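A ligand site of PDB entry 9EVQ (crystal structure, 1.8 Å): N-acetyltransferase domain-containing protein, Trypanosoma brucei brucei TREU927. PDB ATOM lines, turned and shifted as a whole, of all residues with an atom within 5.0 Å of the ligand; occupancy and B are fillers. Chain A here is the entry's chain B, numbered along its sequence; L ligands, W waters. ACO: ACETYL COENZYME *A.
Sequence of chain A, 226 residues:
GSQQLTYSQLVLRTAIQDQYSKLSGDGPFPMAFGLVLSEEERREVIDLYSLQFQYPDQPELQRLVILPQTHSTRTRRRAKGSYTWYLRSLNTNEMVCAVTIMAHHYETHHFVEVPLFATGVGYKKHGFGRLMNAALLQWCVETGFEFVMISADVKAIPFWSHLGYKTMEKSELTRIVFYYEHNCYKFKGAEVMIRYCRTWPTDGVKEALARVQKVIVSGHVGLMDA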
ATOM      1  N   LEU A  10      12.115 -21.644  -7.079  1.00  0.00           N
ATOM      2  CA  LEU A  10      12.707 -21.541  -8.414  1.00  0.00           C
ATOM      3  C   LEU A  10      11.676 -20.973  -9.382  1.00  0.00           C
ATOM      4  O   LEU A  10      10.614 -21.561  -9.610  1.00  0.00           O
ATOM      5  CB  LEU A  10      13.183 -22.903  -8.902  1.00  0.00           C
ATOM      6  CG  LEU A  10      13.793 -22.907 -10.307  1.00  0.00           C
ATOM      7  CD1 LEU A  10      14.994 -21.969 -10.367  1.00  0.00           C
ATOM      8  CD2 LEU A  10      14.204 -24.325 -10.729  1.00  0.00           C
ATOM      9  N   LEU A  12      11.897 -19.755 -13.249  1.00  0.00           N
ATOM     10  CA  LEU A  12      12.740 -19.720 -14.426  1.00  0.00           C
ATOM     11  C   LEU A  12      12.237 -18.673 -15.400  1.00  0.00           C
ATOM     12  O   LEU A  12      11.036 -18.438 -15.529  1.00  0.00           O
ATOM     13  CB  LEU A  12      12.787 -21.075 -15.112  1.00  0.00           C
ATOM     14  CG  LEU A  12      13.547 -22.152 -14.348  1.00  0.00           C
ATOM     15  CD1 LEU A  12      13.334 -23.504 -15.002  1.00  0.00           C
ATOM     16  CD2 LEU A  12      15.035 -21.803 -14.262  1.00  0.00           C
ATOM     17  N   GLN A  52      18.862 -16.264 -16.597  1.00  0.00           N
ATOM     18  CA  GLN A  52      18.238 -17.582 -16.578  1.00  0.00           C
ATOM     19  C   GLN A  52      17.158 -17.722 -15.523  1.00  0.00           C
ATOM     20  O   GLN A  52      16.205 -18.478 -15.716  1.00  0.00           O
ATOM     21  CB  GLN A  52      19.312 -18.667 -16.359  1.00  0.00           C
ATOM     22  CG  GLN A  52      20.432 -18.591 -17.411  1.00  0.00           C
ATOM     23  CD  GLN A  52      19.877 -18.824 -18.795  1.00  0.00           C
ATOM     24  OE1 GLN A  52      18.994 -19.643 -18.969  1.00  0.00           O
ATOM     25  NE2 GLN A  52      20.391 -18.089 -19.773  1.00  0.00           N
ATOM     26  N   PHE A  53      17.264 -16.952 -14.445  1.00  0.00           N
ATOM     27  CA  PHE A  53      16.338 -17.056 -13.323  1.00  0.00           C
ATOM     28  C   PHE A  53      15.539 -15.779 -13.148  1.00  0.00           C
ATOM     29  O   PHE A  53      16.082 -14.676 -13.237  1.00  0.00           O
ATOM     30  CB  PHE A  53      17.097 -17.320 -12.019  1.00  0.00           C
ATOM     31  CG  PHE A  53      17.981 -18.531 -12.061  1.00  0.00           C
ATOM     32  CD1 PHE A  53      17.417 -19.804 -12.080  1.00  0.00           C
ATOM     33  CD2 PHE A  53      19.357 -18.408 -12.075  1.00  0.00           C
ATOM     34  CE1 PHE A  53      18.234 -20.912 -12.105  1.00  0.00           C
ATOM     35  CE2 PHE A  53      20.165 -19.524 -12.108  1.00  0.00           C
ATOM     36  CZ  PHE A  53      19.601 -20.774 -12.134  1.00  0.00           C
ATOM     37  N   VAL A 114      24.234 -27.613  -4.169  1.00  0.00           N
ATOM     38  CA  VAL A 114      24.401 -26.802  -5.382  1.00  0.00           C
ATOM     39  C   VAL A 114      23.232 -25.825  -5.551  1.00  0.00           C
ATOM     40  O   VAL A 114      22.248 -26.175  -6.219  1.00  0.00           O
ATOM     41  CB  VAL A 114      24.539 -27.703  -6.622  1.00  0.00           C
ATOM     42  CG1 VAL A 114      24.893 -26.873  -7.879  1.00  0.00           C
ATOM     43  CG2 VAL A 114      25.567 -28.817  -6.385  1.00  0.00           C
ATOM     44  N   PRO A 115      23.280 -24.620  -4.971  1.00  0.00           N
ATOM     45  CA  PRO A 115      22.112 -23.728  -5.083  1.00  0.00           C
ATOM     46  C   PRO A 115      21.846 -23.222  -6.496  1.00  0.00           C
ATOM     47  O   PRO A 115      20.684 -23.005  -6.836  1.00  0.00           O
ATOM     48  CB  PRO A 115      22.448 -22.565  -4.144  1.00  0.00           C
ATOM     49  CG  PRO A 115      23.429 -23.128  -3.173  1.00  0.00           C
ATOM     50  CD  PRO A 115      24.213 -24.180  -3.902  1.00  0.00           C
ATOM     51  N   LEU A 116      22.885 -23.023  -7.326  1.00  0.00           N
ATOM     52  CA  LEU A 116      22.742 -22.378  -8.632  1.00  0.00           C
ATOM     53  C   LEU A 116      23.565 -23.122  -9.669  1.00  0.00           C
ATOM     54  O   LEU A 116      24.672 -23.561  -9.384  1.00  0.00           O
ATOM     55  CB  LEU A 116      23.209 -20.932  -8.605  1.00  0.00           C
ATOM     56  CG  LEU A 116      22.489 -19.966  -7.659  1.00  0.00           C
ATOM     57  CD1 LEU A 116      23.219 -18.610  -7.544  1.00  0.00           C
ATOM     58  CD2 LEU A 116      21.086 -19.768  -8.135  1.00  0.00           C
ATOM     59  N   PHE A 117      23.021 -23.236 -10.897  1.00  0.00           N
ATOM     60  CA  PHE A 117      23.723 -23.922 -11.978  1.00  0.00           C
ATOM     61  C   PHE A 117      23.049 -23.496 -13.269  1.00  0.00           C
ATOM     62  O   PHE A 117      21.831 -23.642 -13.407  1.00  0.00           O
ATOM     63  CB  PHE A 117      23.660 -25.431 -11.800  1.00  0.00           C
ATOM     64  CG  PHE A 117      24.453 -26.219 -12.798  1.00  0.00           C
ATOM     65  CD1 PHE A 117      23.997 -26.378 -14.111  1.00  0.00           C
ATOM     66  CD2 PHE A 117      25.637 -26.850 -12.429  1.00  0.00           C
ATOM     67  CE1 PHE A 117      24.724 -27.117 -15.028  1.00  0.00           C
ATOM     68  CE2 PHE A 117      26.359 -27.608 -13.346  1.00  0.00           C
ATOM     69  CZ  PHE A 117      25.911 -27.739 -14.645  1.00  0.00           C
ATOM     70  N   ALA A 118      23.823 -22.975 -14.230  1.00  0.00           N
ATOM     71  CA  ALA A 118      23.168 -22.514 -15.449  1.00  0.00           C
ATOM     72  C   ALA A 118      24.189 -22.417 -16.572  1.00  0.00           C
ATOM     73  O   ALA A 118      25.382 -22.182 -16.336  1.00  0.00           O
ATOM     74  CB  ALA A 118      22.487 -21.158 -15.230  1.00  0.00           C
ATOM     75  N   THR A 119      23.714 -22.615 -17.787  1.00  0.00           N
ATOM     76  CA  THR A 119      24.492 -22.330 -18.975  1.00  0.00           C
ATOM     77  C   THR A 119      23.964 -21.043 -19.610  1.00  0.00           C
ATOM     78  O   THR A 119      22.787 -20.696 -19.476  1.00  0.00           O
ATOM     79  CB  THR A 119      24.436 -23.503 -19.952  1.00  0.00           C
ATOM     80  OG1 THR A 119      25.015 -24.669 -19.327  1.00  0.00           O
ATOM     81  CG2 THR A 119      25.240 -23.193 -21.208  1.00  0.00           C
ATOM     82  N   TYR A 123      24.991 -20.593 -25.600  1.00  0.00           N
ATOM     83  CA  TYR A 123      25.869 -21.726 -25.324  1.00  0.00           C
ATOM     84  C   TYR A 123      25.096 -22.965 -24.931  1.00  0.00           C
ATOM     85  O   TYR A 123      25.713 -23.951 -24.502  1.00  0.00           O
ATOM     86  CB  TYR A 123      26.865 -21.367 -24.222  1.00  0.00           C
ATOM     87  CG  TYR A 123      27.744 -20.190 -24.601  1.00  0.00           C
ATOM     88  CD1 TYR A 123      28.759 -20.337 -25.518  1.00  0.00           C
ATOM     89  CD2 TYR A 123      27.521 -18.936 -24.060  1.00  0.00           C
ATOM     90  CE1 TYR A 123      29.556 -19.282 -25.874  1.00  0.00           C
ATOM     91  CE2 TYR A 123      28.302 -17.856 -24.410  1.00  0.00           C
ATOM     92  CZ  TYR A 123      29.329 -18.037 -25.320  1.00  0.00           C
ATOM     93  OH  TYR A 123      30.140 -16.987 -25.689  1.00  0.00           O
ATOM     94  N   LYS A 124      23.774 -22.966 -25.062  1.00  0.00           N
ATOM     95  CA  LYS A 124      22.978 -24.096 -24.621  1.00  0.00           C
ATOM     96  C   LYS A 124      23.055 -25.266 -25.589  1.00  0.00           C
ATOM     97  O   LYS A 124      23.338 -25.105 -26.782  1.00  0.00           O
ATOM     98  CB  LYS A 124      21.522 -23.657 -24.427  1.00  0.00           C
ATOM     99  CG  LYS A 124      21.365 -22.898 -23.104  1.00  0.00           C
ATOM    100  CD  LYS A 124      20.129 -22.051 -23.064  1.00  0.00           C
ATOM    101  CE  LYS A 124      20.193 -21.126 -21.868  1.00  0.00           C
ATOM    102  NZ  LYS A 124      20.179 -21.880 -20.594  1.00  0.00           N
ATOM    103  N   LYS A 125      22.821 -26.450 -25.047  1.00  0.00           N
ATOM    104  CA  LYS A 125      22.786 -27.685 -25.831  1.00  0.00           C
ATOM    105  C   LYS A 125      24.105 -27.957 -26.544  1.00  0.00           C
ATOM    106  O   LYS A 125      24.113 -28.499 -27.657  1.00  0.00           O
ATOM    107  CB  LYS A 125      21.620 -27.672 -26.823  1.00  0.00           C
ATOM    108  CG  LYS A 125      20.256 -27.700 -26.113  1.00  0.00           C
ATOM    109  CD  LYS A 125      20.109 -28.968 -25.254  1.00  0.00           C
ATOM    110  CE  LYS A 125      18.767 -29.066 -24.514  1.00  0.00           C
ATOM    111  NZ  LYS A 125      18.549 -28.022 -23.450  1.00  0.00           N
ATOM    112  N   HIS A 126      25.235 -27.576 -25.922  1.00  0.00           N
ATOM    113  CA  HIS A 126      26.559 -27.885 -26.437  1.00  0.00           C
ATOM    114  C   HIS A 126      27.333 -28.865 -25.565  1.00  0.00           C
ATOM    115  O   HIS A 126      28.453 -29.231 -25.923  1.00  0.00           O
ATOM    116  CB  HIS A 126      27.421 -26.636 -26.554  1.00  0.00           C
ATOM    117  CG  HIS A 126      27.065 -25.754 -27.710  1.00  0.00           C
ATOM    118  ND1 HIS A 126      26.035 -24.834 -27.650  1.00  0.00           N
ATOM    119  CD2 HIS A 126      27.601 -25.647 -28.943  1.00  0.00           C
ATOM    120  CE1 HIS A 126      25.963 -24.193 -28.816  1.00  0.00           C
ATOM    121  NE2 HIS A 126      26.900 -24.673 -29.611  1.00  0.00           N
ATOM    122  N   GLY A 127      26.781 -29.247 -24.419  1.00  0.00           N
ATOM    123  CA  GLY A 127      27.479 -30.090 -23.474  1.00  0.00           C
ATOM    124  C   GLY A 127      28.142 -29.373 -22.315  1.00  0.00           C
ATOM    125  O   GLY A 127      28.818 -30.029 -21.527  1.00  0.00           O
ATOM    126  N   PHE A 128      27.974 -28.053 -22.204  1.00  0.00           N
ATOM    127  CA  PHE A 128      28.652 -27.349 -21.116  1.00  0.00           C
ATOM    128  C   PHE A 128      28.029 -27.673 -19.762  1.00  0.00           C
ATOM    129  O   PHE A 128      28.717 -27.618 -18.738  1.00  0.00           O
ATOM    130  CB  PHE A 128      28.641 -25.849 -21.340  1.00  0.00           C
ATOM    131  CG  PHE A 128      29.478 -25.415 -22.524  1.00  0.00           C
ATOM    132  CD1 PHE A 128      30.846 -25.612 -22.525  1.00  0.00           C
ATOM    133  CD2 PHE A 128      28.876 -24.826 -23.619  1.00  0.00           C
ATOM    134  CE1 PHE A 128      31.618 -25.202 -23.621  1.00  0.00           C
ATOM    135  CE2 PHE A 128      29.633 -24.412 -24.702  1.00  0.00           C
ATOM    136  CZ  PHE A 128      31.008 -24.612 -24.709  1.00  0.00           C
ATOM    137  N   GLY A 129      26.725 -27.975 -19.736  1.00  0.00           N
ATOM    138  CA  GLY A 129      26.105 -28.382 -18.474  1.00  0.00           C
ATOM    139  C   GLY A 129      26.691 -29.673 -17.955  1.00  0.00           C
ATOM    140  O   GLY A 129      27.077 -29.782 -16.789  1.00  0.00           O
ATOM    141  N   ARG A 130      26.763 -30.688 -18.810  1.00  0.00           N
ATOM    142  CA  ARG A 130      27.400 -31.930 -18.401  1.00  0.00           C
ATOM    143  C   ARG A 130      28.864 -31.695 -18.005  1.00  0.00           C
ATOM    144  O   ARG A 130      29.348 -32.256 -17.017  1.00  0.00           O
ATOM    145  CB  ARG A 130      27.299 -32.961 -19.515  1.00  0.00           C
ATOM    146  CG  ARG A 130      27.909 -34.308 -19.165  1.00  0.00           C
ATOM    147  CD  ARG A 130      27.816 -35.277 -20.335  1.00  0.00           C
ATOM    148  NE  ARG A 130      26.458 -35.733 -20.653  1.00  0.00           N
ATOM    149  CZ  ARG A 130      25.758 -36.605 -19.929  1.00  0.00           C
ATOM    150  NH1 ARG A 130      26.267 -37.104 -18.812  1.00  0.00           N
ATOM    151  NH2 ARG A 130      24.543 -36.976 -20.330  1.00  0.00           N
ATOM    152  N   LEU A 131      29.581 -30.848 -18.764  1.00  0.00           N
ATOM    153  CA  LEU A 131      30.981 -30.624 -18.464  1.00  0.00           C
ATOM    154  C   LEU A 131      31.176 -29.991 -17.096  1.00  0.00           C
ATOM    155  O   LEU A 131      32.011 -30.434 -16.304  1.00  0.00           O
ATOM    156  CB  LEU A 131      31.611 -29.744 -19.540  1.00  0.00           C
ATOM    157  CG  LEU A 131      33.059 -29.335 -19.244  1.00  0.00           C
ATOM    158  CD1 LEU A 131      33.970 -30.547 -19.150  1.00  0.00           C
ATOM    159  CD2 LEU A 131      33.518 -28.424 -20.396  1.00  0.00           C
ATOM    160  N   LYS A 155      10.963 -28.438 -11.938  1.00  0.00           N
ATOM    161  CA  LYS A 155      11.464 -28.172 -13.272  1.00  0.00           C
ATOM    162  C   LYS A 155      12.911 -28.618 -13.473  1.00  0.00           C
ATOM    163  O   LYS A 155      13.343 -28.743 -14.628  1.00  0.00           O
ATOM    164  CB  LYS A 155      11.324 -26.683 -13.604  1.00  0.00           C
ATOM    165  CG  LYS A 155       9.856 -26.285 -13.758  1.00  0.00           C
ATOM    166  CD  LYS A 155       9.677 -24.915 -14.370  1.00  0.00           C
ATOM    167  CE  LYS A 155       8.360 -24.850 -15.181  1.00  0.00           C
ATOM    168  NZ  LYS A 155       7.131 -25.201 -14.406  1.00  0.00           N
ATOM    169  N   ALA A 156      13.655 -28.863 -12.404  1.00  0.00           N
ATOM    170  CA  ALA A 156      15.068 -29.228 -12.501  1.00  0.00           C
ATOM    171  C   ALA A 156      15.332 -30.718 -12.366  1.00  0.00           C
ATOM    172  O   ALA A 156      16.379 -31.197 -12.814  1.00  0.00           O
ATOM    173  CB  ALA A 156      15.882 -28.492 -11.425  1.00  0.00           C
ATOM    174  N   PRO A 158      14.322 -33.398 -14.004  1.00  0.00           N
ATOM    175  CA  PRO A 158      14.716 -34.199 -15.191  1.00  0.00           C
ATOM    176  C   PRO A 158      16.163 -33.995 -15.576  1.00  0.00           C
ATOM    177  O   PRO A 158      16.827 -34.944 -16.029  1.00  0.00           O
ATOM    178  CB  PRO A 158      13.751 -33.711 -16.275  1.00  0.00           C
ATOM    179  CG  PRO A 158      12.569 -33.189 -15.503  1.00  0.00           C
ATOM    180  CD  PRO A 158      13.211 -32.508 -14.311  1.00  0.00           C
ATOM    181  N   PHE A 159      16.674 -32.772 -15.433  1.00  0.00           N
ATOM    182  CA  PHE A 159      18.066 -32.469 -15.772  1.00  0.00           C
ATOM    183  C   PHE A 159      19.037 -33.195 -14.837  1.00  0.00           C
ATOM    184  O   PHE A 159      19.904 -33.954 -15.277  1.00  0.00           O
ATOM    185  CB  PHE A 159      18.304 -30.965 -15.711  1.00  0.00           C
ATOM    186  CG  PHE A 159      19.757 -30.569 -15.876  1.00  0.00           C
ATOM    187  CD1 PHE A 159      20.396 -30.753 -17.088  1.00  0.00           C
ATOM    188  CD2 PHE A 159      20.461 -30.008 -14.821  1.00  0.00           C
ATOM    189  CE1 PHE A 159      21.727 -30.394 -17.253  1.00  0.00           C
ATOM    190  CE2 PHE A 159      21.788 -29.637 -14.994  1.00  0.00           C
ATOM    191  CZ  PHE A 159      22.411 -29.827 -16.207  1.00  0.00           C
ATOM    192  N   TRP A 160      18.892 -32.971 -13.535  1.00  0.00           N
ATOM    193  CA  TRP A 160      19.761 -33.636 -12.564  1.00  0.00           C
ATOM    194  C   TRP A 160      19.618 -35.156 -12.683  1.00  0.00           C
ATOM    195  O   TRP A 160      20.618 -35.882 -12.638  1.00  0.00           O
ATOM    196  CB  TRP A 160      19.425 -33.181 -11.147  1.00  0.00           C
ATOM    197  CG  TRP A 160      19.691 -31.721 -10.921  1.00  0.00           C
ATOM    198  CD1 TRP A 160      18.780 -30.758 -10.577  1.00  0.00           C
ATOM    199  CD2 TRP A 160      20.951 -31.049 -11.063  1.00  0.00           C
ATOM    200  NE1 TRP A 160      19.401 -29.547 -10.476  1.00  0.00           N
ATOM    201  CE2 TRP A 160      20.735 -29.697 -10.756  1.00  0.00           C
ATOM    202  CE3 TRP A 160      22.245 -31.468 -11.381  1.00  0.00           C
ATOM    203  CZ2 TRP A 160      21.752 -28.747 -10.778  1.00  0.00           C
ATOM    204  CZ3 TRP A 160      23.261 -30.539 -11.382  1.00  0.00           C
ATOM    205  CH2 TRP A 160      23.017 -29.189 -11.092  1.00  0.00           C
ATOM    206  N   HIS A 162      18.855 -36.854 -15.408  1.00  0.00           N
ATOM    207  CA  HIS A 162      19.589 -37.286 -16.593  1.00  0.00           C
ATOM    208  C   HIS A 162      21.084 -37.370 -16.324  1.00  0.00           C
ATOM    209  O   HIS A 162      21.758 -38.291 -16.805  1.00  0.00           O
ATOM    210  CB  HIS A 162      19.296 -36.349 -17.773  1.00  0.00           C
ATOM    211  CG  HIS A 162      19.961 -36.780 -19.048  1.00  0.00           C
ATOM    212  ND1 HIS A 162      19.695 -37.981 -19.656  1.00  0.00           N
ATOM    213  CD2 HIS A 162      20.898 -36.165 -19.813  1.00  0.00           C
ATOM    214  CE1 HIS A 162      20.422 -38.091 -20.749  1.00  0.00           C
ATOM    215  NE2 HIS A 162      21.175 -37.007 -20.859  1.00  0.00           N
ATOM    216  N   LEU A 163      21.641 -36.426 -15.562  1.00  0.00           N
ATOM    217  CA  LEU A 163      23.075 -36.440 -15.289  1.00  0.00           C
ATOM    218  C   LEU A 163      23.458 -37.413 -14.181  1.00  0.00           C
ATOM    219  O   LEU A 163      24.626 -37.424 -13.777  1.00  0.00           O
ATOM    220  CB  LEU A 163      23.587 -35.045 -14.955  1.00  0.00           C
ATOM    221  CG  LEU A 163      23.497 -33.982 -16.057  1.00  0.00           C
ATOM    222  CD1 LEU A 163      24.112 -32.662 -15.589  1.00  0.00           C
ATOM    223  CD2 LEU A 163      24.172 -34.458 -17.338  1.00  0.00           C
ATOM    224  N   PHE A 187      14.664 -25.274  -2.082  1.00  0.00           N
ATOM    225  CA  PHE A 187      13.666 -24.759  -3.013  1.00  0.00           C
ATOM    226  C   PHE A 187      12.279 -25.294  -2.674  1.00  0.00           C
ATOM    227  O   PHE A 187      12.113 -26.463  -2.319  1.00  0.00           O
ATOM    228  CB  PHE A 187      14.038 -25.121  -4.448  1.00  0.00           C
ATOM    229  CG  PHE A 187      15.223 -24.344  -4.991  1.00  0.00           C
ATOM    230  CD1 PHE A 187      15.073 -23.029  -5.403  1.00  0.00           C
ATOM    231  CD2 PHE A 187      16.462 -24.950  -5.115  1.00  0.00           C
ATOM    232  CE1 PHE A 187      16.165 -22.330  -5.903  1.00  0.00           C
ATOM    233  CE2 PHE A 187      17.555 -24.251  -5.629  1.00  0.00           C
ATOM    234  CZ  PHE A 187      17.391 -22.932  -6.028  1.00  0.00           C
ATOM    235  N   ARG A 211      32.972 -34.714 -25.532  1.00  0.00           N
ATOM    236  CA  ARG A 211      31.681 -34.495 -26.163  1.00  0.00           C
ATOM    237  C   ARG A 211      31.384 -33.033 -26.464  1.00  0.00           C
ATOM    238  O   ARG A 211      30.398 -32.746 -27.146  1.00  0.00           O
ATOM    239  CB  ARG A 211      30.576 -35.051 -25.267  1.00  0.00           C
ATOM    240  CG  ARG A 211      30.801 -36.512 -24.985  1.00  0.00           C
ATOM    241  CD  ARG A 211      29.680 -37.042 -24.175  1.00  0.00           C
ATOM    242  NE  ARG A 211      28.419 -36.675 -24.804  1.00  0.00           N
ATOM    243  CZ  ARG A 211      27.236 -36.847 -24.232  1.00  0.00           C
ATOM    244  NH1 ARG A 211      27.172 -37.386 -23.018  1.00  0.00           N
ATOM    245  NH2 ARG A 211      26.140 -36.497 -24.871  1.00  0.00           N
HETATM  246  N1A ACO L   1      15.963 -32.207 -18.789  1.00  0.00           N
HETATM  247  C2A ACO L   1      16.598 -33.315 -19.181  1.00  0.00           C
HETATM  248  N3A ACO L   1      17.743 -33.443 -19.856  1.00  0.00           N
HETATM  249  C4A ACO L   1      18.254 -32.242 -20.146  1.00  0.00           C
HETATM  250  C5A ACO L   1      17.714 -31.004 -19.811  1.00  0.00           C
HETATM  251  C6A ACO L   1      16.506 -31.005 -19.105  1.00  0.00           C
HETATM  252  N6A ACO L   1      15.875 -29.886 -18.713  1.00  0.00           N
HETATM  253  N7A ACO L   1      18.529 -29.984 -20.272  1.00  0.00           N
HETATM  254  C8A ACO L   1      19.520 -30.610 -20.859  1.00  0.00           C
HETATM  255  N9A ACO L   1      19.420 -31.979 -20.826  1.00  0.00           N
HETATM  256  C1B ACO L   1      20.362 -32.957 -21.374  1.00  0.00           C
HETATM  257  C2B ACO L   1      20.910 -32.589 -22.747  1.00  0.00           C
HETATM  258  O2B ACO L   1      20.069 -33.131 -23.761  1.00  0.00           O
HETATM  259  C3B ACO L   1      22.268 -33.285 -22.715  1.00  0.00           C
HETATM  260  O3B ACO L   1      22.080 -34.706 -22.928  1.00  0.00           O
HETATM  261  P3B ACO L   1      23.223 -35.723 -23.456  1.00  0.00           P
HETATM  262  O7A ACO L   1      24.541 -35.314 -22.864  1.00  0.00           O
HETATM  263  O8A ACO L   1      23.188 -35.555 -24.953  1.00  0.00           O
HETATM  264  O9A ACO L   1      22.807 -37.132 -23.075  1.00  0.00           O
HETATM  265  C4B ACO L   1      22.695 -33.162 -21.240  1.00  0.00           C
HETATM  266  O4B ACO L   1      21.467 -33.001 -20.500  1.00  0.00           O
HETATM  267  C5B ACO L   1      23.603 -31.988 -20.951  1.00  0.00           C
HETATM  268  O5B ACO L   1      23.126 -30.881 -21.703  1.00  0.00           O
HETATM  269  P1A ACO L   1      24.064 -29.611 -21.879  1.00  0.00           P
HETATM  270  O1A ACO L   1      24.059 -29.203 -23.325  1.00  0.00           O
HETATM  271  O2A ACO L   1      25.383 -29.820 -21.189  1.00  0.00           O
HETATM  272  O3A ACO L   1      23.249 -28.596 -20.961  1.00  0.00           O
HETATM  273  P2A ACO L   1      22.638 -27.185 -21.347  1.00  0.00           P
HETATM  274  O4A ACO L   1      23.679 -26.284 -21.843  1.00  0.00           O
HETATM  275  O5A ACO L   1      21.383 -27.483 -22.161  1.00  0.00           O
HETATM  276  O6A ACO L   1      22.217 -26.621 -19.935  1.00  0.00           O
HETATM  277  CBP ACO L   1      20.626 -26.260 -18.170  1.00  0.00           C
HETATM  278  CCP ACO L   1      21.182 -27.248 -19.183  1.00  0.00           C
HETATM  279  CDP ACO L   1      19.520 -26.961 -17.366  1.00  0.00           C
HETATM  280  CEP ACO L   1      21.766 -25.825 -17.236  1.00  0.00           C
HETATM  281  CAP ACO L   1      20.047 -25.018 -18.908  1.00  0.00           C
HETATM  282  OAP ACO L   1      18.805 -25.334 -19.551  1.00  0.00           O
HETATM  283  C9P ACO L   1      19.877 -23.861 -17.932  1.00  0.00           C
HETATM  284  O9P ACO L   1      20.839 -23.173 -17.633  1.00  0.00           O
HETATM  285  N8P ACO L   1      18.653 -23.665 -17.440  1.00  0.00           N
HETATM  286  C7P ACO L   1      18.348 -22.539 -16.572  1.00  0.00           C
HETATM  287  C6P ACO L   1      18.842 -22.748 -15.150  1.00  0.00           C
HETATM  288  C5P ACO L   1      18.353 -24.065 -14.604  1.00  0.00           C
HETATM  289  O5P ACO L   1      17.237 -24.469 -14.871  1.00  0.00           O
HETATM  290  N4P ACO L   1      19.214 -24.754 -13.846  1.00  0.00           N
HETATM  291  C3P ACO L   1      18.996 -26.157 -13.537  1.00  0.00           C
HETATM  292  C2P ACO L   1      18.946 -26.519 -12.060  1.00  0.00           C
HETATM  293  S1P ACO L   1      18.044 -25.173 -11.246  1.00  0.00           S
HETATM  294  C   ACO L   1      19.291 -24.796 -10.071  1.00  0.00           C
HETATM  295  O   ACO L   1      19.885 -25.643  -9.452  1.00  0.00           O
HETATM  296  CH3 ACO L   1      19.560 -23.324  -9.951  1.00  0.00           C
HETATM  297  O   HOH W   1      23.733 -39.384 -23.315  1.00  0.00           O
HETATM  298  O   HOH W   2      21.385 -33.817 -26.063  1.00  0.00           O
HETATM  299  O   HOH W   3      18.891 -35.850 -23.696  1.00  0.00           O
HETATM  300  O   HOH W   4      25.688 -26.400 -23.331  1.00  0.00           O
HETATM  301  O   HOH W   5      17.848 -23.350 -20.944  1.00  0.00           O
HETATM  302  O   HOH W   6      17.678 -36.044 -21.226  1.00  0.00           O
HETATM  303  O   HOH W   7      23.358 -37.518 -26.760  1.00  0.00           O
HETATM  304  O   HOH W   8      15.963 -24.905 -17.239  1.00  0.00           O
HETATM  305  O   HOH W   9      18.269 -27.668  -8.472  1.00  0.00           O
HETATM  306  O   HOH W  10      20.519 -37.794 -24.214  1.00  0.00           O
HETATM  307  O   HOH W  11      16.352 -26.979 -19.286  1.00  0.00           O
HETATM  308  O   HOH W  12      16.288 -28.243 -22.226  1.00  0.00           O
HETATM  309  O   HOH W  13      23.910 -31.080 -25.174  1.00  0.00           O
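Residues that only touch the ligand: Ala 118 (3.3 Å), Pro 115 (3.3 Å), Phe 53 (3.4 Å), Trp 160 (3.4 Å), Leu 12 (3.5 Å), Pro 158 (3.6 Å), Leu 116 (3.6 Å), Ala 156 (3.7 Å), Gln 52 (3.8 Å) and Leu 10 (3.97 Å).
Hydrophobic or aromatic side chains that line the ligand: Leu 10, Leu 12, Phe 53, Phe 117, Ala 118, Ala 156, Pro 158, Phe 159, Trp 160 and His 162.
Within 4 Å of the ligand: Leu 10, Leu 12, Gln 52, Phe 53, Pro 115, Leu 116, Phe 117, Ala 118, Thr 119, Lys 124, Lys 125, His 126, Gly 127, Phe 128, Gly 129, Arg 130, Ala 156, Pro 158, Phe 159, Trp 160, His 162 and Arg 211.
The nearest printed residue that does not touch the ligand is Val 114 (4.04 Å).
N4P of the ligand lies within hydrogen-bond range of O of Phe 117, 2.9 Å away.
The side-chain amino group (NZ) of Lys 125 is in salt-bridge range of an oxygen (O5A) of the ligand (3.2 Å).
O9A of the ligand sits at hydrogen-bond distance from NE2 of His 162, at 2.8 Å.
The backbone NH (N) of Arg 130 lies within hydrogen-bond range of an oxygen (O2A) of the ligand, at 2.9 Å.
N of Thr 119 is in hydrogen-bond range of O9P of the ligand, 2.9 Å away.
The side-chain hydroxyl (OG1) of Thr 119 lies within hydrogen-bond range of an oxygen (O4A) of the ligand, 3.3 Å away.
The backbone NH of Gly 127 sits at hydrogen-bond distance from an oxygen (O1A) of the ligand (2.9 Å).
N of Gly 129 lies within hydrogen-bond range of O2A of the ligand (2.7 Å).
O7A of the ligand lies within salt-bridge range of NH2 of Arg 211, 2.8 Å away.
The backbone NH of Phe 128 is in hydrogen-bond range of an oxygen (O2A) of the ligand (3.3 Å).
N of His 126 lies within hydrogen-bond range of O1A of the ligand, 3.3 Å away.
The side-chain amino group (NZ) of Lys 124 sits at hydrogen-bond distance from an oxygen (O9P) of the ligand (3.3 Å).
The backbone NH (N) of Lys 125 lies within hydrogen-bond range of an oxygen (O4A) of the ligand, at 3.3 Å.
The backbone NH (N) of Phe 159 is in hydrogen-bond range of a nitrogen (N1A) of the ligand, at 3.5 Å.
NE of Arg 130 lies within salt-bridge range of O7A of the ligand, at 3.0 Å.
A ring nitrogen (ND1) of His 126 lies within hydrogen-bond range of the backbone carbonyl oxygen (O) of Tyr 123, at 3.3 Å.
The side-chain amino group (NZ) of Lys 124 sits at hydrogen-bond distance from the side-chain amide oxygen (OE1) of Gln 52, 3.0 Å away.
The side-chain amino group (NZ) of Lys 124 lies within hydrogen-bond range of the backbone carbonyl oxygen (O) of Thr 119, 3.1 Å away.
NE2 of His 162 lies within hydrogen-bond range of NH2 of Arg 130, 3.4 Å away.
The backbone carbonyl oxygen of Lys 124 lies within hydrogen-bond range of a ring nitrogen (ND1) of His 126 (2.8 Å).
Water W5 lies within hydrogen-bond range of OAP of the ligand and NZ of Lys 124.
Water W13 lies within hydrogen-bond range of an oxygen (O1A) of the ligand (2.6 Å) and the backbone NH (N) of Gly 127 (3.5 Å).
Water W9 lies within hydrogen-bond range of O of the ligand (2.8 Å) and NE1 of Trp 160 (3.0 Å).
Water W6 bridges a nitrogen (N3A) of the ligand (2.9 Å) and a ring nitrogen (ND1) of His 162 (3.2 Å).
Water W12 bridges the side-chain amino group of Lys 125 (2.6 Å) and a nitrogen (N7A) of the ligand (3.4 Å).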
